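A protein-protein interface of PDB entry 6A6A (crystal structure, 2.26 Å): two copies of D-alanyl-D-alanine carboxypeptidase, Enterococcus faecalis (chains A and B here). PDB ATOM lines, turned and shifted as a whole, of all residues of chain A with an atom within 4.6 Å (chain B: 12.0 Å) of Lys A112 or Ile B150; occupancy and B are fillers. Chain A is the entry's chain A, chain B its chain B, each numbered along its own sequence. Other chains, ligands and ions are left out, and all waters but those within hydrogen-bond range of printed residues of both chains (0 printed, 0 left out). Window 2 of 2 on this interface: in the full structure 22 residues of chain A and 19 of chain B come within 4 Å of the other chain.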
ATOM      1  N   ASP A 105       5.970  12.179 -24.853  1.00  0.00           N
ATOM      2  CA  ASP A 105       6.424  13.562 -25.030  1.00  0.00           C
ATOM      3  C   ASP A 105       7.758  13.781 -24.299  1.00  0.00           C
ATOM      4  O   ASP A 105       8.644  14.518 -24.778  1.00  0.00           O
ATOM      5  CB  ASP A 105       5.401  14.568 -24.505  1.00  0.00           C
ATOM      6  CG  ASP A 105       4.076  14.603 -25.235  1.00  0.00           C
ATOM      7  OD1 ASP A 105       3.975  14.003 -26.320  1.00  0.00           O
ATOM      8  OD2 ASP A 105       3.154  15.234 -24.696  1.00  0.00           O
ATOM      9  N   VAL A 108      10.326  12.313 -26.386  1.00  0.00           N
ATOM     10  CA  VAL A 108      10.636  13.227 -27.511  1.00  0.00           C
ATOM     11  C   VAL A 108      11.562  14.366 -27.032  1.00  0.00           C
ATOM     12  O   VAL A 108      12.544  14.691 -27.693  1.00  0.00           O
ATOM     13  CB  VAL A 108       9.364  13.735 -28.213  1.00  0.00           C
ATOM     14  CG1 VAL A 108       9.684  14.769 -29.289  1.00  0.00           C
ATOM     15  CG2 VAL A 108       8.593  12.581 -28.830  1.00  0.00           C
ATOM     16  N   ALA A 109      11.272  14.922 -25.858  1.00  0.00           N
ATOM     17  CA  ALA A 109      12.034  16.012 -25.282  1.00  0.00           C
ATOM     18  C   ALA A 109      13.508  15.600 -25.129  1.00  0.00           C
ATOM     19  O   ALA A 109      14.403  16.384 -25.458  1.00  0.00           O
ATOM     20  CB  ALA A 109      11.419  16.432 -23.957  1.00  0.00           C
ATOM     21  N   GLU A 110      13.738  14.380 -24.617  1.00  0.00           N
ATOM     22  CA  GLU A 110      15.069  13.793 -24.446  1.00  0.00           C
ATOM     23  C   GLU A 110      15.822  13.769 -25.784  1.00  0.00           C
ATOM     24  O   GLU A 110      17.009  14.081 -25.830  1.00  0.00           O
ATOM     25  CB  GLU A 110      14.996  12.358 -23.935  1.00  0.00           C
ATOM     26  CG  GLU A 110      14.576  12.233 -22.481  1.00  0.00           C
ATOM     27  CD  GLU A 110      14.277  10.798 -22.052  1.00  0.00           C
ATOM     28  OE1 GLU A 110      13.675  10.044 -22.842  1.00  0.00           O
ATOM     29  OE2 GLU A 110      14.652  10.431 -20.938  1.00  0.00           O
ATOM     30  N   TYR A 111      15.144  13.392 -26.874  1.00  0.00           N
ATOM     31  CA  TYR A 111      15.843  13.311 -28.149  1.00  0.00           C
ATOM     32  C   TYR A 111      16.070  14.713 -28.731  1.00  0.00           C
ATOM     33  O   TYR A 111      17.107  14.917 -29.322  1.00  0.00           O
ATOM     34  CB  TYR A 111      15.163  12.347 -29.116  1.00  0.00           C
ATOM     35  CG  TYR A 111      15.580  10.905 -28.941  1.00  0.00           C
ATOM     36  CD1 TYR A 111      16.814  10.450 -29.392  1.00  0.00           C
ATOM     37  CD2 TYR A 111      14.727   9.979 -28.357  1.00  0.00           C
ATOM     38  CE1 TYR A 111      17.204   9.127 -29.247  1.00  0.00           C
ATOM     39  CE2 TYR A 111      15.103   8.652 -28.201  1.00  0.00           C
ATOM     40  CZ  TYR A 111      16.340   8.219 -28.658  1.00  0.00           C
ATOM     41  OH  TYR A 111      16.688   6.899 -28.532  1.00  0.00           O
ATOM     42  N   LYS A 112      15.155  15.673 -28.516  1.00  0.00           N
ATOM     43  CA  LYS A 112      15.386  17.061 -28.958  1.00  0.00           C
ATOM     44  C   LYS A 112      16.658  17.588 -28.287  1.00  0.00           C
ATOM     45  O   LYS A 112      17.458  18.218 -28.930  1.00  0.00           O
ATOM     46  CB  LYS A 112      14.217  17.998 -28.633  1.00  0.00           C
ATOM     47  CG  LYS A 112      12.910  17.681 -29.336  1.00  0.00           C
ATOM     48  CD  LYS A 112      11.875  18.776 -29.238  1.00  0.00           C
ATOM     49  CE  LYS A 112      11.259  18.902 -27.862  1.00  0.00           C
ATOM     50  NZ  LYS A 112      10.386  20.098 -27.774  1.00  0.00           N
ATOM     51  N   ALA A 113      16.840  17.270 -26.997  1.00  0.00           N
ATOM     52  CA  ALA A 113      17.972  17.766 -26.181  1.00  0.00           C
ATOM     53  C   ALA A 113      19.287  17.091 -26.583  1.00  0.00           C
ATOM     54  O   ALA A 113      20.375  17.517 -26.146  1.00  0.00           O
ATOM     55  CB  ALA A 113      17.696  17.542 -24.710  1.00  0.00           C
ATOM     56  N   LYS A 114      19.203  16.027 -27.392  1.00  0.00           N
ATOM     57  CA  LYS A 114      20.401  15.321 -27.809  1.00  0.00           C
ATOM     58  C   LYS A 114      20.779  15.714 -29.239  1.00  0.00           C
ATOM     59  O   LYS A 114      21.757  15.213 -29.750  1.00  0.00           O
ATOM     60  CB  LYS A 114      20.214  13.816 -27.586  1.00  0.00           C
ATOM     61  CG  LYS A 114      20.119  13.432 -26.119  1.00  0.00           C
ATOM     62  CD  LYS A 114      19.908  11.927 -25.902  1.00  0.00           C
ATOM     63  CE  LYS A 114      19.835  11.524 -24.442  1.00  0.00           C
ATOM     64  NZ  LYS A 114      19.606  10.067 -24.305  1.00  0.00           N
ATOM     65  N   GLY A 115      20.021  16.641 -29.844  1.00  0.00           N
ATOM     66  CA  GLY A 115      20.342  17.224 -31.128  1.00  0.00           C
ATOM     67  C   GLY A 115      19.406  16.775 -32.243  1.00  0.00           C
ATOM     68  O   GLY A 115      19.806  16.694 -33.413  1.00  0.00           O
ATOM     69  N   TYR A 116      18.146  16.516 -31.901  1.00  0.00           N
ATOM     70  CA  TYR A 116      17.157  16.048 -32.852  1.00  0.00           C
ATOM     71  C   TYR A 116      16.121  17.153 -33.083  1.00  0.00           C
ATOM     72  O   TYR A 116      15.597  17.706 -32.136  1.00  0.00           O
ATOM     73  CB  TYR A 116      16.501  14.771 -32.322  1.00  0.00           C
ATOM     74  CG  TYR A 116      17.385  13.551 -32.362  1.00  0.00           C
ATOM     75  CD1 TYR A 116      18.522  13.459 -31.586  1.00  0.00           C
ATOM     76  CD2 TYR A 116      17.087  12.488 -33.191  1.00  0.00           C
ATOM     77  CE1 TYR A 116      19.339  12.343 -31.632  1.00  0.00           C
ATOM     78  CE2 TYR A 116      17.891  11.363 -33.253  1.00  0.00           C
ATOM     79  CZ  TYR A 116      19.024  11.291 -32.472  1.00  0.00           C
ATOM     80  OH  TYR A 116      19.819  10.189 -32.515  1.00  0.00           O
ATOM     81  N   SER A 118      12.314  18.132 -33.796  1.00  0.00           N
ATOM     82  CA  SER A 118      11.188  17.472 -33.167  1.00  0.00           C
ATOM     83  C   SER A 118      10.654  16.385 -34.102  1.00  0.00           C
ATOM     84  O   SER A 118      10.168  15.381 -33.612  1.00  0.00           O
ATOM     85  CB  SER A 118      10.116  18.428 -32.745  1.00  0.00           C
ATOM     86  OG  SER A 118       9.736  19.232 -33.824  1.00  0.00           O
ATOM     87  N   ALA A 121      12.991  13.510 -33.500  1.00  0.00           N
ATOM     88  CA  ALA A 121      12.828  13.062 -32.146  1.00  0.00           C
ATOM     89  C   ALA A 121      11.594  12.154 -32.040  1.00  0.00           C
ATOM     90  O   ALA A 121      11.649  11.146 -31.327  1.00  0.00           O
ATOM     91  CB  ALA A 121      12.729  14.257 -31.231  1.00  0.00           C
ATOM     92  N   ARG B  82      -1.421  27.038 -18.779  1.00  0.00           N
ATOM     93  CA  ARG B  82      -1.734  26.827 -20.172  1.00  0.00           C
ATOM     94  C   ARG B  82      -2.045  28.193 -20.807  1.00  0.00           C
ATOM     95  O   ARG B  82      -1.532  28.484 -21.883  1.00  0.00           O
ATOM     96  CB  ARG B  82      -2.847  25.781 -20.283  1.00  0.00           C
ATOM     97  CG  ARG B  82      -2.403  24.355 -19.957  1.00  0.00           C
ATOM     98  CD  ARG B  82      -3.477  23.352 -20.355  1.00  0.00           C
ATOM     99  NE  ARG B  82      -3.512  22.087 -19.610  1.00  0.00           N
ATOM    100  CZ  ARG B  82      -2.626  21.087 -19.730  1.00  0.00           C
ATOM    101  NH1 ARG B  82      -2.917  19.904 -19.228  1.00  0.00           N
ATOM    102  NH2 ARG B  82      -1.444  21.274 -20.306  1.00  0.00           N
ATOM    103  N   GLY B  85       0.731  30.033 -21.933  1.00  0.00           N
ATOM    104  CA  GLY B  85       1.483  29.320 -22.971  1.00  0.00           C
ATOM    105  C   GLY B  85       2.474  28.315 -22.398  1.00  0.00           C
ATOM    106  O   GLY B  85       3.338  27.844 -23.110  1.00  0.00           O
ATOM    107  N   VAL B  86       2.333  27.992 -21.107  1.00  0.00           N
ATOM    108  CA  VAL B  86       3.206  27.078 -20.382  1.00  0.00           C
ATOM    109  C   VAL B  86       2.440  25.769 -20.154  1.00  0.00           C
ATOM    110  O   VAL B  86       1.284  25.795 -19.775  1.00  0.00           O
ATOM    111  CB  VAL B  86       3.671  27.727 -19.059  1.00  0.00           C
ATOM    112  CG1 VAL B  86       4.259  26.714 -18.092  1.00  0.00           C
ATOM    113  CG2 VAL B  86       4.652  28.880 -19.298  1.00  0.00           C
ATOM    114  N   TYR B  87       3.118  24.633 -20.356  1.00  0.00           N
ATOM    115  CA  TYR B  87       2.463  23.323 -20.536  1.00  0.00           C
ATOM    116  C   TYR B  87       3.060  22.317 -19.563  1.00  0.00           C
ATOM    117  O   TYR B  87       4.008  21.605 -19.905  1.00  0.00           O
ATOM    118  CB  TYR B  87       2.524  22.841 -21.994  1.00  0.00           C
ATOM    119  CG  TYR B  87       1.624  23.645 -22.893  1.00  0.00           C
ATOM    120  CD1 TYR B  87       2.031  24.876 -23.385  1.00  0.00           C
ATOM    121  CD2 TYR B  87       0.343  23.216 -23.202  1.00  0.00           C
ATOM    122  CE1 TYR B  87       1.199  25.651 -24.175  1.00  0.00           C
ATOM    123  CE2 TYR B  87      -0.502  23.976 -23.997  1.00  0.00           C
ATOM    124  CZ  TYR B  87      -0.074  25.198 -24.485  1.00  0.00           C
ATOM    125  OH  TYR B  87      -0.893  25.965 -25.268  1.00  0.00           O
ATOM    126  N   PRO B  88       2.448  22.222 -18.358  1.00  0.00           N
ATOM    127  CA  PRO B  88       2.876  21.313 -17.308  1.00  0.00           C
ATOM    128  C   PRO B  88       2.121  19.976 -17.346  1.00  0.00           C
ATOM    129  O   PRO B  88       1.069  19.862 -17.953  1.00  0.00           O
ATOM    130  CB  PRO B  88       2.522  22.091 -16.036  1.00  0.00           C
ATOM    131  CG  PRO B  88       1.453  23.112 -16.455  1.00  0.00           C
ATOM    132  CD  PRO B  88       1.241  22.942 -17.941  1.00  0.00           C
ATOM    133  N   ILE B  89       2.707  18.966 -16.703  1.00  0.00           N
ATOM    134  CA  ILE B  89       2.060  17.685 -16.476  1.00  0.00           C
ATOM    135  C   ILE B  89       2.264  17.317 -15.006  1.00  0.00           C
ATOM    136  O   ILE B  89       3.280  17.709 -14.380  1.00  0.00           O
ATOM    137  CB  ILE B  89       2.635  16.606 -17.420  1.00  0.00           C
ATOM    138  CG1 ILE B  89       4.144  16.436 -17.220  1.00  0.00           C
ATOM    139  CG2 ILE B  89       2.280  16.913 -18.876  1.00  0.00           C
ATOM    140  CD1 ILE B  89       4.628  15.006 -17.333  1.00  0.00           C
ATOM    141  N   ASN B 146       6.085  18.579 -14.103  1.00  0.00           N
ATOM    142  CA  ASN B 146       7.119  18.662 -15.136  1.00  0.00           C
ATOM    143  C   ASN B 146       6.513  19.291 -16.400  1.00  0.00           C
ATOM    144  O   ASN B 146       5.301  19.510 -16.501  1.00  0.00           O
ATOM    145  CB  ASN B 146       7.740  17.288 -15.451  1.00  0.00           C
ATOM    146  CG  ASN B 146       8.471  16.669 -14.278  1.00  0.00           C
ATOM    147  OD1 ASN B 146       8.657  17.303 -13.245  1.00  0.00           O
ATOM    148  ND2 ASN B 146       8.878  15.420 -14.422  1.00  0.00           N
ATOM    149  N   ALA B 147       7.369  19.570 -17.379  1.00  0.00           N
ATOM    150  CA  ALA B 147       6.928  20.094 -18.640  1.00  0.00           C
ATOM    151  C   ALA B 147       6.299  18.958 -19.464  1.00  0.00           C
ATOM    152  O   ALA B 147       6.618  17.798 -19.265  1.00  0.00           O
ATOM    153  CB  ALA B 147       8.104  20.739 -19.328  1.00  0.00           C
ATOM    154  N   ASP B 148       5.391  19.294 -20.380  1.00  0.00           N
ATOM    155  CA  ASP B 148       4.805  18.279 -21.283  1.00  0.00           C
ATOM    156  C   ASP B 148       5.803  17.876 -22.380  1.00  0.00           C
ATOM    157  O   ASP B 148       5.441  17.134 -23.269  1.00  0.00           O
ATOM    158  CB  ASP B 148       3.505  18.751 -21.947  1.00  0.00           C
ATOM    159  CG  ASP B 148       3.718  19.664 -23.141  1.00  0.00           C
ATOM    160  OD1 ASP B 148       4.843  20.186 -23.282  1.00  0.00           O
ATOM    161  OD2 ASP B 148       2.754  19.845 -23.916  1.00  0.00           O
ATOM    162  N   GLY B 149       7.024  18.424 -22.347  1.00  0.00           N
ATOM    163  CA  GLY B 149       8.089  18.005 -23.222  1.00  0.00           C
ATOM    164  C   GLY B 149       8.161  18.831 -24.489  1.00  0.00           C
ATOM    165  O   GLY B 149       9.170  19.485 -24.726  1.00  0.00           O
ATOM    166  N   ILE B 150       7.088  18.805 -25.290  1.00  0.00           N
ATOM    167  CA  ILE B 150       7.126  19.274 -26.684  1.00  0.00           C
ATOM    168  C   ILE B 150       6.591  20.707 -26.829  1.00  0.00           C
ATOM    169  O   ILE B 150       6.758  21.291 -27.880  1.00  0.00           O
ATOM    170  CB  ILE B 150       6.385  18.301 -27.625  1.00  0.00           C
ATOM    171  CG1 ILE B 150       4.912  18.112 -27.249  1.00  0.00           C
ATOM    172  CG2 ILE B 150       7.124  16.968 -27.692  1.00  0.00           C
ATOM    173  CD1 ILE B 150       4.039  17.631 -28.395  1.00  0.00           C
ATOM    174  N   HIS B 151       5.919  21.243 -25.805  1.00  0.00           N
ATOM    175  CA  HIS B 151       5.420  22.622 -25.817  1.00  0.00           C
ATOM    176  C   HIS B 151       6.261  23.497 -24.888  1.00  0.00           C
ATOM    177  O   HIS B 151       6.475  24.654 -25.167  1.00  0.00           O
ATOM    178  CB  HIS B 151       3.950  22.688 -25.400  1.00  0.00           C
ATOM    179  CG  HIS B 151       3.011  22.063 -26.375  1.00  0.00           C
ATOM    180  ND1 HIS B 151       2.633  20.736 -26.288  1.00  0.00           N
ATOM    181  CD2 HIS B 151       2.354  22.580 -27.436  1.00  0.00           C
ATOM    182  CE1 HIS B 151       1.792  20.459 -27.261  1.00  0.00           C
ATOM    183  NE2 HIS B 151       1.602  21.575 -27.980  1.00  0.00           N
ATOM    184  N   SER B 152       6.742  22.902 -23.810  1.00  0.00           N
ATOM    185  CA  SER B 152       7.565  23.645 -22.836  1.00  0.00           C
ATOM    186  C   SER B 152       8.716  22.776 -22.338  1.00  0.00           C
ATOM    187  O   SER B 152       8.654  21.559 -22.473  1.00  0.00           O
ATOM    188  CB  SER B 152       6.743  24.119 -21.667  1.00  0.00           C
ATOM    189  OG  SER B 152       5.427  24.457 -22.037  1.00  0.00           O
ATOM    190  N   THR B 153       9.757  23.427 -21.843  1.00  0.00           N
ATOM    191  CA  THR B 153      10.886  22.730 -21.191  1.00  0.00           C
ATOM    192  C   THR B 153      10.661  22.714 -19.678  1.00  0.00           C
ATOM    193  O   THR B 153       9.888  23.529 -19.180  1.00  0.00           O
ATOM    194  CB  THR B 153      12.246  23.310 -21.587  1.00  0.00           C
ATOM    195  OG1 THR B 153      12.785  24.116 -20.546  1.00  0.00           O
ATOM    196  CG2 THR B 153      12.191  24.112 -22.859  1.00  0.00           C
ATOM    197  N   GLY B 154      11.379  21.853 -18.963  1.00  0.00           N
ATOM    198  CA  GLY B 154      11.175  21.758 -17.513  1.00  0.00           C
ATOM    199  C   GLY B 154      11.430  23.095 -16.855  1.00  0.00           C
ATOM    200  O   GLY B 154      10.531  23.546 -16.188  1.00  0.00           O
ATOM    201  N   ASN B 155      12.508  23.780 -17.243  1.00  0.00           N
ATOM    202  CA  ASN B 155      12.918  25.076 -16.656  1.00  0.00           C
ATOM    203  C   ASN B 155      11.831  26.127 -16.845  1.00  0.00           C
ATOM    204  O   ASN B 155      11.607  26.848 -15.921  1.00  0.00           O
ATOM    205  CB  ASN B 155      14.203  25.577 -17.298  1.00  0.00           C
ATOM    206  CG  ASN B 155      15.337  24.615 -17.075  1.00  0.00           C
ATOM    207  OD1 ASN B 155      15.616  24.265 -15.938  1.00  0.00           O
ATOM    208  ND2 ASN B 155      15.973  24.176 -18.146  1.00  0.00           N
ATOM    209  N   GLU B 156      11.197  26.177 -18.006  1.00  0.00           N
ATOM    210  CA  GLU B 156      10.120  27.161 -18.249  1.00  0.00           C
ATOM    211  C   GLU B 156       8.966  26.910 -17.282  1.00  0.00           C
ATOM    212  O   GLU B 156       8.402  27.863 -16.791  1.00  0.00           O
ATOM    213  CB  GLU B 156       9.549  26.968 -19.637  1.00  0.00           C
ATOM    214  CG  GLU B 156      10.447  27.443 -20.749  1.00  0.00           C
ATOM    215  CD  GLU B 156       9.903  27.069 -22.113  1.00  0.00           C
ATOM    216  OE1 GLU B 156       8.803  26.552 -22.178  1.00  0.00           O
ATOM    217  OE2 GLU B 156      10.581  27.311 -23.091  1.00  0.00           O
ATOM    218  N   VAL B 157       8.660  25.648 -17.033  1.00  0.00           N
ATOM    219  CA  VAL B 157       7.591  25.279 -16.146  1.00  0.00           C
ATOM    220  C   VAL B 157       8.053  25.574 -14.714  1.00  0.00           C
ATOM    221  O   VAL B 157       7.329  26.177 -13.915  1.00  0.00           O
ATOM    222  CB  VAL B 157       7.169  23.811 -16.367  1.00  0.00           C
ATOM    223  CG1 VAL B 157       6.346  23.266 -15.204  1.00  0.00           C
ATOM    224  CG2 VAL B 157       6.422  23.645 -17.678  1.00  0.00           C
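The backbone carbonyl oxygen of Gly B149 lies within hydrogen-bond range of the side-chain amino group of Lys A112, at 3.3 Å.
The side-chain carboxylate of Asp A105 sits close to the backbone carbonyl oxygen of Asp B148 (3.3 Å).
O of Tyr B87 sits at hydrogen-bond distance from N of Asp B148 (2.7 Å).
The side-chain carboxylate (OD1) of Asp B148 lies close to the backbone NH (N) of Ile B150 (3.3 Å).
The side-chain carboxylate of Asp B148 is in hydrogen-bond range of a ring nitrogen (ND1) of His B151, at 2.5 Å.
The side-chain carboxylate (OD1) of Asp B148 is in hydrogen-bond range of the backbone NH (N) of Ser B152, at 3.4 Å.
Among the printed residues, merely in contact across the chains: Asp A105 with Gly B149 (3.9 Å), Val A108 with Ile B150 (3.7 Å), Ala A109 with Gly B149 (3.8 Å) and Lys A112 with Ile B150 (3.5 Å).
Asp A105 touches two residues of chain B.
Of chain B, only Ile B150 (3.7 Å) comes within 4 Å of Val A108.
Ala A109 touches just one residue of chain B: Gly B149.
Lys A112 touches two residues of chain B.
No residue of chain B comes within 4 Å of Ala A113.
Lys A114 touches none of the printed residues of chain B.
No residue of chain B comes within 4 Å of Gly A115.
No residue of chain B comes within 4 Å of Ser A118.
Printed residues of chain A within 4 Å of Asp B148: Asp A105 (2.8 Å).
Of the printed residues of chain A, Gly B149 touches Asp A105 (3.9 Å), Ala A109 (3.8 Å) and Lys A112 (3.3 Å).
Ile B150 touches two residues of chain A.
Glu B156 touches none of the printed residues of chain A.
Of the 12 printed residues of chain A, 4 touch a printed residue of chain B.
Of the 18 printed residues of chain B, 3 touch a printed residue of chain A.
Printed residues of chain B that touch a printed residue of chain A: Asp B148, Gly B149 and Ile B150.
Hydrophobic or aromatic side chains of chain B that line the printed part of chain A: Ile B150.
Among the printed residues, 6 pairs touch across the chains.
Among the printed residues, no Asp or Glu carboxylate lies within 4 Å of a Lys or Arg side-chain nitrogen of the other chain.
No position is printed for both chains.
Of the 6 pairs that touch across the chains among the printed residues, none has its exchanged pair printed and touching as well.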
